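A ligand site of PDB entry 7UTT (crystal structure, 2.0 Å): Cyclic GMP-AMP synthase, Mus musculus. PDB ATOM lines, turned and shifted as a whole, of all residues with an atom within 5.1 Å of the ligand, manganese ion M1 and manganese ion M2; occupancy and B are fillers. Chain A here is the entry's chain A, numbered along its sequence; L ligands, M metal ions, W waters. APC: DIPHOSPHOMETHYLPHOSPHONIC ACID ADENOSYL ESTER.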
ATOM      1  N   THR A  54      22.106 -13.653  15.013  1.00  0.00           N
ATOM      2  CA  THR A  54      20.999 -13.721  14.055  1.00  0.00           C
ATOM      3  C   THR A  54      19.992 -12.589  14.310  1.00  0.00           C
ATOM      4  O   THR A  54      20.165 -11.758  15.203  1.00  0.00           O
ATOM      5  CB  THR A  54      20.255 -15.089  14.139  1.00  0.00           C
ATOM      6  OG1 THR A  54      19.738 -15.238  15.455  1.00  0.00           O
ATOM      7  CG2 THR A  54      21.153 -16.221  13.922  1.00  0.00           C
ATOM      8  N   GLY A  55      18.916 -12.556  13.509  1.00  0.00           N
ATOM      9  CA  GLY A  55      17.850 -11.617  13.735  1.00  0.00           C
ATOM     10  C   GLY A  55      18.156 -10.266  13.150  1.00  0.00           C
ATOM     11  O   GLY A  55      19.191 -10.085  12.476  1.00  0.00           O
ATOM     12  N   SER A  56      17.248  -9.298  13.397  1.00  0.00           N
ATOM     13  CA  SER A  56      17.232  -8.069  12.612  1.00  0.00           C
ATOM     14  C   SER A  56      18.496  -7.229  12.703  1.00  0.00           C
ATOM     15  O   SER A  56      18.866  -6.541  11.728  1.00  0.00           O
ATOM     16  CB  SER A  56      16.032  -7.205  12.971  1.00  0.00           C
ATOM     17  OG  SER A  56      16.050  -6.836  14.349  1.00  0.00           O
ATOM     18  N   GLU A  59      21.096  -8.661  10.433  1.00  0.00           N
ATOM     19  CA  GLU A  59      20.604  -8.532   9.058  1.00  0.00           C
ATOM     20  C   GLU A  59      20.531  -7.090   8.564  1.00  0.00           C
ATOM     21  O   GLU A  59      20.138  -6.844   7.437  1.00  0.00           O
ATOM     22  CB  GLU A  59      19.194  -9.163   8.987  1.00  0.00           C
ATOM     23  CG  GLU A  59      19.201 -10.661   9.298  1.00  0.00           C
ATOM     24  CD  GLU A  59      17.818 -11.235   9.527  1.00  0.00           C
ATOM     25  OE1 GLU A  59      16.880 -10.493   9.903  1.00  0.00           O
ATOM     26  OE2 GLU A  59      17.656 -12.460   9.293  1.00  0.00           O
ATOM     27  N   VAL A  61      18.329  -4.869   9.462  1.00  0.00           N
ATOM     28  CA  VAL A  61      16.946  -4.380   9.353  1.00  0.00           C
ATOM     29  C   VAL A  61      16.329  -4.060  10.734  1.00  0.00           C
ATOM     30  O   VAL A  61      15.134  -3.914  10.840  1.00  0.00           O
ATOM     31  CB  VAL A  61      16.048  -5.324   8.513  1.00  0.00           C
ATOM     32  CG1 VAL A  61      16.545  -5.378   7.073  1.00  0.00           C
ATOM     33  CG2 VAL A  61      16.031  -6.722   9.078  1.00  0.00           C
ATOM     34  N   LYS A  62      17.165  -3.886  11.772  1.00  0.00           N
ATOM     35  CA  LYS A  62      16.680  -3.376  13.050  1.00  0.00           C
ATOM     36  C   LYS A  62      16.314  -1.908  12.856  1.00  0.00           C
ATOM     37  O   LYS A  62      17.062  -1.157  12.231  1.00  0.00           O
ATOM     38  CB  LYS A  62      17.753  -3.471  14.130  1.00  0.00           C
ATOM     39  CG  LYS A  62      17.262  -3.040  15.514  1.00  0.00           C
ATOM     40  CD  LYS A  62      16.462  -4.139  16.180  1.00  0.00           C
ATOM     41  CE  LYS A  62      15.914  -3.727  17.534  1.00  0.00           C
ATOM     42  NZ  LYS A  62      15.076  -2.515  17.502  1.00  0.00           N
ATOM     43  N   GLU A  68      17.513  -4.546  20.727  1.00  0.00           N
ATOM     44  CA  GLU A  68      17.155  -5.959  20.792  1.00  0.00           C
ATOM     45  C   GLU A  68      18.040  -6.822  19.895  1.00  0.00           C
ATOM     46  O   GLU A  68      18.064  -6.652  18.674  1.00  0.00           O
ATOM     47  CB  GLU A  68      15.647  -6.151  20.482  1.00  0.00           C
ATOM     48  CG  GLU A  68      15.021  -7.424  21.046  1.00  0.00           C
ATOM     49  CD  GLU A  68      15.110  -8.609  20.141  1.00  0.00           C
ATOM     50  OE1 GLU A  68      15.611  -8.454  18.988  1.00  0.00           O
ATOM     51  OE2 GLU A  68      14.665  -9.721  20.544  1.00  0.00           O
ATOM     52  N   PHE A  69      18.778  -7.725  20.529  1.00  0.00           N
ATOM     53  CA  PHE A  69      19.804  -8.520  19.885  1.00  0.00           C
ATOM     54  C   PHE A  69      19.490  -9.982  20.085  1.00  0.00           C
ATOM     55  O   PHE A  69      19.100 -10.358  21.192  1.00  0.00           O
ATOM     56  CB  PHE A  69      21.185  -8.225  20.515  1.00  0.00           C
ATOM     57  CG  PHE A  69      21.705  -6.844  20.274  1.00  0.00           C
ATOM     58  CD1 PHE A  69      21.233  -5.768  21.004  1.00  0.00           C
ATOM     59  CD2 PHE A  69      22.731  -6.626  19.357  1.00  0.00           C
ATOM     60  CE1 PHE A  69      21.743  -4.502  20.816  1.00  0.00           C
ATOM     61  CE2 PHE A  69      23.263  -5.354  19.171  1.00  0.00           C
ATOM     62  CZ  PHE A  69      22.737  -4.278  19.884  1.00  0.00           C
ATOM     63  N   ASP A  70      19.662 -10.783  19.027  1.00  0.00           N
ATOM     64  CA  ASP A  70      19.457 -12.227  19.056  1.00  0.00           C
ATOM     65  C   ASP A  70      20.745 -13.013  18.792  1.00  0.00           C
ATOM     66  O   ASP A  70      21.464 -12.725  17.838  1.00  0.00           O
ATOM     67  CB  ASP A  70      18.413 -12.596  18.014  1.00  0.00           C
ATOM     68  CG  ASP A  70      17.163 -11.795  18.188  1.00  0.00           C
ATOM     69  OD1 ASP A  70      16.511 -12.009  19.235  1.00  0.00           O
ATOM     70  OD2 ASP A  70      16.858 -10.932  17.299  1.00  0.00           O
ATOM     71  N   ASP A 164      18.351 -11.882  23.547  1.00  0.00           N
ATOM     72  CA  ASP A 164      17.782 -13.217  23.552  1.00  0.00           C
ATOM     73  C   ASP A 164      18.919 -14.211  23.289  1.00  0.00           C
ATOM     74  O   ASP A 164      19.490 -14.213  22.213  1.00  0.00           O
ATOM     75  CB  ASP A 164      16.723 -13.354  22.448  1.00  0.00           C
ATOM     76  CG  ASP A 164      15.411 -12.642  22.806  1.00  0.00           C
ATOM     77  OD1 ASP A 164      15.242 -12.204  23.982  1.00  0.00           O
ATOM     78  OD2 ASP A 164      14.551 -12.509  21.917  1.00  0.00           O
ATOM     79  N   ARG A 221      11.426 -27.162  17.907  1.00  0.00           N
ATOM     80  CA  ARG A 221      10.946 -26.496  16.665  1.00  0.00           C
ATOM     81  C   ARG A 221      12.141 -26.175  15.758  1.00  0.00           C
ATOM     82  O   ARG A 221      13.207 -25.773  16.281  1.00  0.00           O
ATOM     83  CB  ARG A 221      10.176 -25.229  17.064  1.00  0.00           C
ATOM     84  CG  ARG A 221       9.475 -24.516  15.907  1.00  0.00           C
ATOM     85  CD  ARG A 221       9.485 -23.019  16.110  1.00  0.00           C
ATOM     86  NE  ARG A 221      10.663 -22.477  15.484  1.00  0.00           N
ATOM     87  CZ  ARG A 221      11.348 -21.421  15.868  1.00  0.00           C
ATOM     88  NH1 ARG A 221      11.025 -20.737  16.951  1.00  0.00           N
ATOM     89  NH2 ARG A 221      12.392 -21.052  15.169  1.00  0.00           N
ATOM     90  N   LEU A 222      11.947 -26.320  14.448  1.00  0.00           N
ATOM     91  CA  LEU A 222      12.973 -26.027  13.441  1.00  0.00           C
ATOM     92  C   LEU A 222      13.262 -24.565  13.363  1.00  0.00           C
ATOM     93  O   LEU A 222      12.339 -23.762  13.423  1.00  0.00           O
ATOM     94  CB  LEU A 222      12.547 -26.530  12.037  1.00  0.00           C
ATOM     95  CG  LEU A 222      12.456 -28.035  11.830  1.00  0.00           C
ATOM     96  CD1 LEU A 222      11.947 -28.423  10.429  1.00  0.00           C
ATOM     97  CD2 LEU A 222      13.840 -28.615  12.045  1.00  0.00           C
ATOM     98  N   SER A 223      14.559 -24.201  13.274  1.00  0.00           N
ATOM     99  CA  SER A 223      15.000 -22.819  13.050  1.00  0.00           C
ATOM    100  C   SER A 223      15.926 -22.752  11.845  1.00  0.00           C
ATOM    101  O   SER A 223      16.863 -23.570  11.719  1.00  0.00           O
ATOM    102  CB  SER A 223      15.783 -22.296  14.230  1.00  0.00           C
ATOM    103  OG  SER A 223      16.277 -21.005  13.955  1.00  0.00           O
ATOM    104  N   SER A 225      17.263 -19.541  11.039  1.00  0.00           N
ATOM    105  CA  SER A 225      17.658 -18.165  11.270  1.00  0.00           C
ATOM    106  C   SER A 225      18.974 -17.837  10.584  1.00  0.00           C
ATOM    107  O   SER A 225      19.165 -16.714  10.118  1.00  0.00           O
ATOM    108  CB  SER A 225      17.761 -17.886  12.794  1.00  0.00           C
ATOM    109  OG  SER A 225      17.640 -16.535  12.985  1.00  0.00           O
ATOM    110  N   GLU A 228      18.023 -17.463   6.813  1.00  0.00           N
ATOM    111  CA  GLU A 228      17.352 -16.182   6.708  1.00  0.00           C
ATOM    112  C   GLU A 228      18.322 -15.008   6.703  1.00  0.00           C
ATOM    113  O   GLU A 228      18.187 -14.100   5.911  1.00  0.00           O
ATOM    114  CB  GLU A 228      16.323 -16.047   7.821  1.00  0.00           C
ATOM    115  CG  GLU A 228      15.163 -17.030   7.704  1.00  0.00           C
ATOM    116  CD  GLU A 228      14.248 -17.008   8.924  1.00  0.00           C
ATOM    117  OE1 GLU A 228      14.355 -16.026   9.703  1.00  0.00           O
ATOM    118  OE2 GLU A 228      13.469 -17.982   9.096  1.00  0.00           O
ATOM    119  N   LYS A 259       7.693  -3.461   9.072  1.00  0.00           N
ATOM    120  CA  LYS A 259       7.965  -3.749  10.478  1.00  0.00           C
ATOM    121  C   LYS A 259       7.518  -2.601  11.362  1.00  0.00           C
ATOM    122  O   LYS A 259       6.927  -2.819  12.404  1.00  0.00           O
ATOM    123  CB  LYS A 259       9.440  -4.008  10.764  1.00  0.00           C
ATOM    124  CG  LYS A 259      10.009  -5.257  10.166  1.00  0.00           C
ATOM    125  CD  LYS A 259      11.544  -5.146  10.028  1.00  0.00           C
ATOM    126  CE  LYS A 259      12.290  -4.862  11.363  1.00  0.00           C
ATOM    127  NZ  LYS A 259      12.148  -5.997  12.264  1.00  0.00           N
ATOM    128  N   GLU A 263       4.910  -2.588  14.437  1.00  0.00           N
ATOM    129  CA  GLU A 263       5.438  -2.172  15.758  1.00  0.00           C
ATOM    130  C   GLU A 263       4.563  -1.052  16.358  1.00  0.00           C
ATOM    131  O   GLU A 263       4.172  -1.107  17.519  1.00  0.00           O
ATOM    132  CB  GLU A 263       6.927  -1.708  15.746  1.00  0.00           C
ATOM    133  CG  GLU A 263       8.011  -2.818  15.596  1.00  0.00           C
ATOM    134  CD  GLU A 263       9.492  -2.360  15.878  1.00  0.00           C
ATOM    135  OE1 GLU A 263       9.673  -1.283  16.527  1.00  0.00           O
ATOM    136  OE2 GLU A 263      10.501  -3.067  15.445  1.00  0.00           O
ATOM    137  N   SER A 277       6.891  -9.674  14.316  1.00  0.00           N
ATOM    138  CA  SER A 277       7.621  -9.213  13.147  1.00  0.00           C
ATOM    139  C   SER A 277       7.945 -10.361  12.166  1.00  0.00           C
ATOM    140  O   SER A 277       8.051 -10.149  10.944  1.00  0.00           O
ATOM    141  CB  SER A 277       8.888  -8.448  13.545  1.00  0.00           C
ATOM    142  OG  SER A 277       9.778  -9.307  14.214  1.00  0.00           O
ATOM    143  N   TYR A 278       8.042 -11.597  12.680  1.00  0.00           N
ATOM    144  CA  TYR A 278       8.335 -12.790  11.835  1.00  0.00           C
ATOM    145  C   TYR A 278       7.203 -13.023  10.816  1.00  0.00           C
ATOM    146  O   TYR A 278       7.452 -13.578   9.755  1.00  0.00           O
ATOM    147  CB  TYR A 278       8.584 -14.035  12.681  1.00  0.00           C
ATOM    148  CG  TYR A 278       9.181 -15.158  11.864  1.00  0.00           C
ATOM    149  CD1 TYR A 278      10.475 -15.068  11.394  1.00  0.00           C
ATOM    150  CD2 TYR A 278       8.444 -16.296  11.546  1.00  0.00           C
ATOM    151  CE1 TYR A 278      11.030 -16.093  10.640  1.00  0.00           C
ATOM    152  CE2 TYR A 278       8.974 -17.319  10.752  1.00  0.00           C
ATOM    153  CZ  TYR A 278      10.289 -17.208  10.312  1.00  0.00           C
ATOM    154  OH  TYR A 278      10.881 -18.202   9.582  1.00  0.00           O
ATOM    155  N   LYS A 281       8.265 -10.676   8.072  1.00  0.00           N
ATOM    156  CA  LYS A 281       9.466 -11.238   7.442  1.00  0.00           C
ATOM    157  C   LYS A 281       9.095 -12.365   6.490  1.00  0.00           C
ATOM    158  O   LYS A 281       9.600 -12.473   5.340  1.00  0.00           O
ATOM    159  CB  LYS A 281      10.478 -11.719   8.496  1.00  0.00           C
ATOM    160  CG  LYS A 281      11.868 -11.993   7.957  1.00  0.00           C
ATOM    161  CD  LYS A 281      12.750 -12.602   9.040  1.00  0.00           C
ATOM    162  CE  LYS A 281      14.238 -12.436   8.687  1.00  0.00           C
ATOM    163  NZ  LYS A 281      15.161 -13.194   9.597  1.00  0.00           N
ATOM    164  N   HIS A 324       4.736 -20.844   6.236  1.00  0.00           N
ATOM    165  CA  HIS A 324       6.121 -20.761   6.644  1.00  0.00           C
ATOM    166  C   HIS A 324       6.978 -20.935   5.398  1.00  0.00           C
ATOM    167  O   HIS A 324       6.681 -21.793   4.563  1.00  0.00           O
ATOM    168  CB  HIS A 324       6.380 -21.893   7.642  1.00  0.00           C
ATOM    169  CG  HIS A 324       7.629 -21.746   8.420  1.00  0.00           C
ATOM    170  ND1 HIS A 324       8.878 -21.940   7.857  1.00  0.00           N
ATOM    171  CD2 HIS A 324       7.837 -21.434   9.713  1.00  0.00           C
ATOM    172  CE1 HIS A 324       9.797 -21.722   8.777  1.00  0.00           C
ATOM    173  NE2 HIS A 324       9.192 -21.418   9.917  1.00  0.00           N
HETATM  174  PG  APC L   1      12.926  -7.577  15.429  1.00  0.00           P
HETATM  175  O1G APC L   1      13.461  -6.268  14.917  1.00  0.00           O
HETATM  176  O2G APC L   1      11.432  -7.538  15.488  1.00  0.00           O
HETATM  177  O3G APC L   1      13.624  -8.059  16.689  1.00  0.00           O
HETATM  178  PB  APC L   1      13.535 -10.125  14.389  1.00  0.00           P
HETATM  179  O1B APC L   1      14.910 -10.207  14.957  1.00  0.00           O
HETATM  180  O2B APC L   1      13.618 -10.872  13.059  1.00  0.00           O
HETATM  181  O3B APC L   1      13.200  -8.588  14.194  1.00  0.00           O
HETATM  182  PA  APC L   1      12.917 -11.967  16.858  1.00  0.00           P
HETATM  183  O1A APC L   1      13.941 -11.278  17.718  1.00  0.00           O
HETATM  184  O2A APC L   1      11.675 -12.316  17.589  1.00  0.00           O
HETATM  185  C3A APC L   1      12.782 -10.957  15.572  1.00  0.00           C
HETATM  186  O5' APC L   1      13.582 -13.306  16.236  1.00  0.00           O
HETATM  187  C5' APC L   1      14.955 -13.484  15.885  1.00  0.00           C
HETATM  188  C4' APC L   1      15.097 -14.477  14.733  1.00  0.00           C
HETATM  189  O4' APC L   1      14.715 -15.799  15.163  1.00  0.00           O
HETATM  190  C3' APC L   1      14.202 -14.124  13.525  1.00  0.00           C
HETATM  191  O3' APC L   1      14.841 -13.148  12.669  1.00  0.00           O
HETATM  192  C2' APC L   1      14.027 -15.504  12.920  1.00  0.00           C
HETATM  193  O2' APC L   1      15.172 -15.853  12.129  1.00  0.00           O
HETATM  194  C1' APC L   1      13.959 -16.439  14.123  1.00  0.00           C
HETATM  195  N9  APC L   1      12.558 -16.661  14.574  1.00  0.00           N
HETATM  196  C8  APC L   1      11.887 -15.965  15.519  1.00  0.00           C
HETATM  197  N7  APC L   1      10.633 -16.460  15.652  1.00  0.00           N
HETATM  198  C5  APC L   1      10.533 -17.487  14.761  1.00  0.00           C
HETATM  199  C6  APC L   1       9.507 -18.387  14.445  1.00  0.00           C
HETATM  200  N6  APC L   1       8.297 -18.327  15.067  1.00  0.00           N
HETATM  201  N1  APC L   1       9.719 -19.305  13.488  1.00  0.00           N
HETATM  202  C2  APC L   1      10.901 -19.391  12.838  1.00  0.00           C
HETATM  203  N3  APC L   1      11.910 -18.551  13.136  1.00  0.00           N
HETATM  204  C4  APC L   1      11.742 -17.606  14.095  1.00  0.00           C
HETATM  205 MN    MN M   1      14.474 -11.675  19.796  1.00  0.00          MN
HETATM  206 MN    MN M   2      15.261  -9.480  17.115  1.00  0.00          MN
HETATM  207  O   HOH W   1      16.947  -7.956  16.527  1.00  0.00           O
HETATM  208  O   HOH W   2      12.130  -8.745  19.039  1.00  0.00           O
HETATM  209  O   HOH W   3      14.521  -9.644  10.730  1.00  0.00           O
HETATM  210  O   HOH W   4      14.429 -19.327  15.755  1.00  0.00           O
HETATM  211  O   HOH W   5      13.704 -19.773  11.195  1.00  0.00           O
HETATM  212  O   HOH W   6      13.993 -13.701  19.476  1.00  0.00           O
HETATM  213  O   HOH W   7      12.324 -11.492  20.064  1.00  0.00           O
HETATM  214  O   HOH W   8      13.366  -3.674  15.078  1.00  0.00           O
HETATM  215  O   HOH W   9      11.210 -10.741  12.078  1.00  0.00           O
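The side-chain hydroxyl of Ser 56 lies within hydrogen-bond range of an oxygen (O1G) of the ligand. N3 of the ligand lies close to NH2 of Arg 221 (3.3 Å). O3' of the ligand is in hydrogen-bond range of NZ of Lys 281 (3.1 Å). The side-chain amino group (NZ) of Lys 259 lies within salt-bridge range of an oxygen (O1G) of the ligand (3.0 Å). O1B of the ligand lies close to N of Ser 56 (3.0 Å). The side-chain hydroxyl (OG) of Ser 277 sits at hydrogen-bond distance from an oxygen (O2G) of the ligand, 2.7 Å away. OG of Ser 225 lies within hydrogen-bond range of O2' of the ligand (2.7 Å). An oxygen (O2') of the ligand is in hydrogen-bond range of the side-chain carboxylate (OE1) of Glu 228 (2.6 Å).
O of Ser 56 is in hydrogen-bond range of N of Val 61 (2.9 Å). The side-chain hydroxyl (OH) of Tyr 278 sits at hydrogen-bond distance from the side-chain carboxylate (OE2) of Glu 228 (2.6 Å). The backbone carbonyl oxygen (O) of Asp 70 lies within hydrogen-bond range of the backbone NH (N) of Thr 54 (3.0 Å). O of Ser 56 is in hydrogen-bond range of N of Lys 62, 3.2 Å away. N of Asp 164 is in hydrogen-bond range of O of Phe 69, at 2.9 Å. OG of Ser 225 lies close to OG1 of Thr 54, at 3.5 Å. The side-chain carboxylate (OE2) of Glu 59 lies within salt-bridge range of the side-chain amino group (NZ) of Lys 281 (2.6 Å). The side-chain carboxylate (OE1) of Glu 228 is in salt-bridge range of the side-chain amino group (NZ) of Lys 281 (2.9 Å).
Residues that only touch the ligand: Tyr 278, Gly 55, Lys 62 and His 324. Hydrophobic or aromatic side chains that line the ligand: Tyr 278. The nearest printed residue that does not touch the ligand is Glu 59 (4.3 Å).
Three residues have an atom within 4 Å of manganese ion M1: Glu 68, Asp 70 and Asp 164.
Merely in contact with manganese ion M2: Ser 56. Of the 21 residues printed, 3 come within 4 Å of manganese ion M2. The nearest printed residue that does not touch manganese ion M2 is Gly 55 (4.8 Å).
Manganese ion M1 is bound by OE2 of Glu 68 (2.1 Å), water W6 (2.1 Å), OD1 of Asp 70 (2.1 Å), water W7 (2.2 Å), O1A of the ligand (2.2 Å) and OD2 of Asp 164 (2.3 Å). Manganese ion M1 has six donor atoms within binding distance.
The side-chain carboxylate (OE1) of Glu 68 binds manganese ion M2 (2.2 Å). Manganese ion M2 is bound by the side-chain carboxylate (OD2) of Asp 70. Manganese ion M2 is bound by O3G of the ligand, 2.2 Å away. O1B of the ligand is bound to manganese ion M2, at 2.3 Å. Manganese ion M2 is bound by O1A of the ligand, 2.3 Å away. Water W1 is bound to manganese ion M2. Manganese ion M2 has six donor atoms within binding distance.
Water W1 lies within hydrogen-bond range of OG of Ser 56 and O of Glu 68. Water W8 lies within hydrogen-bond range of an oxygen (O1G) of the ligand (2.6 Å), the side-chain carboxylate of Glu 263 (3.0 Å) and the side-chain amino group of Lys 62 (3.2 Å). Water W9 lies within hydrogen-bond range of O2B of the ligand, OG of Ser 277 and N of Tyr 278. Water W3 bridges OE1 of Glu 59 (2.6 Å) and O2B of the ligand (2.8 Å). Water W5 bridges the side-chain carboxylate of Glu 228 and a nitrogen (N3) of the ligand. Water W4 bridges the guanidinium group (NH2) of Arg 221 (2.7 Å) and the side-chain hydroxyl (OG) of Ser 223 (3.1 Å).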
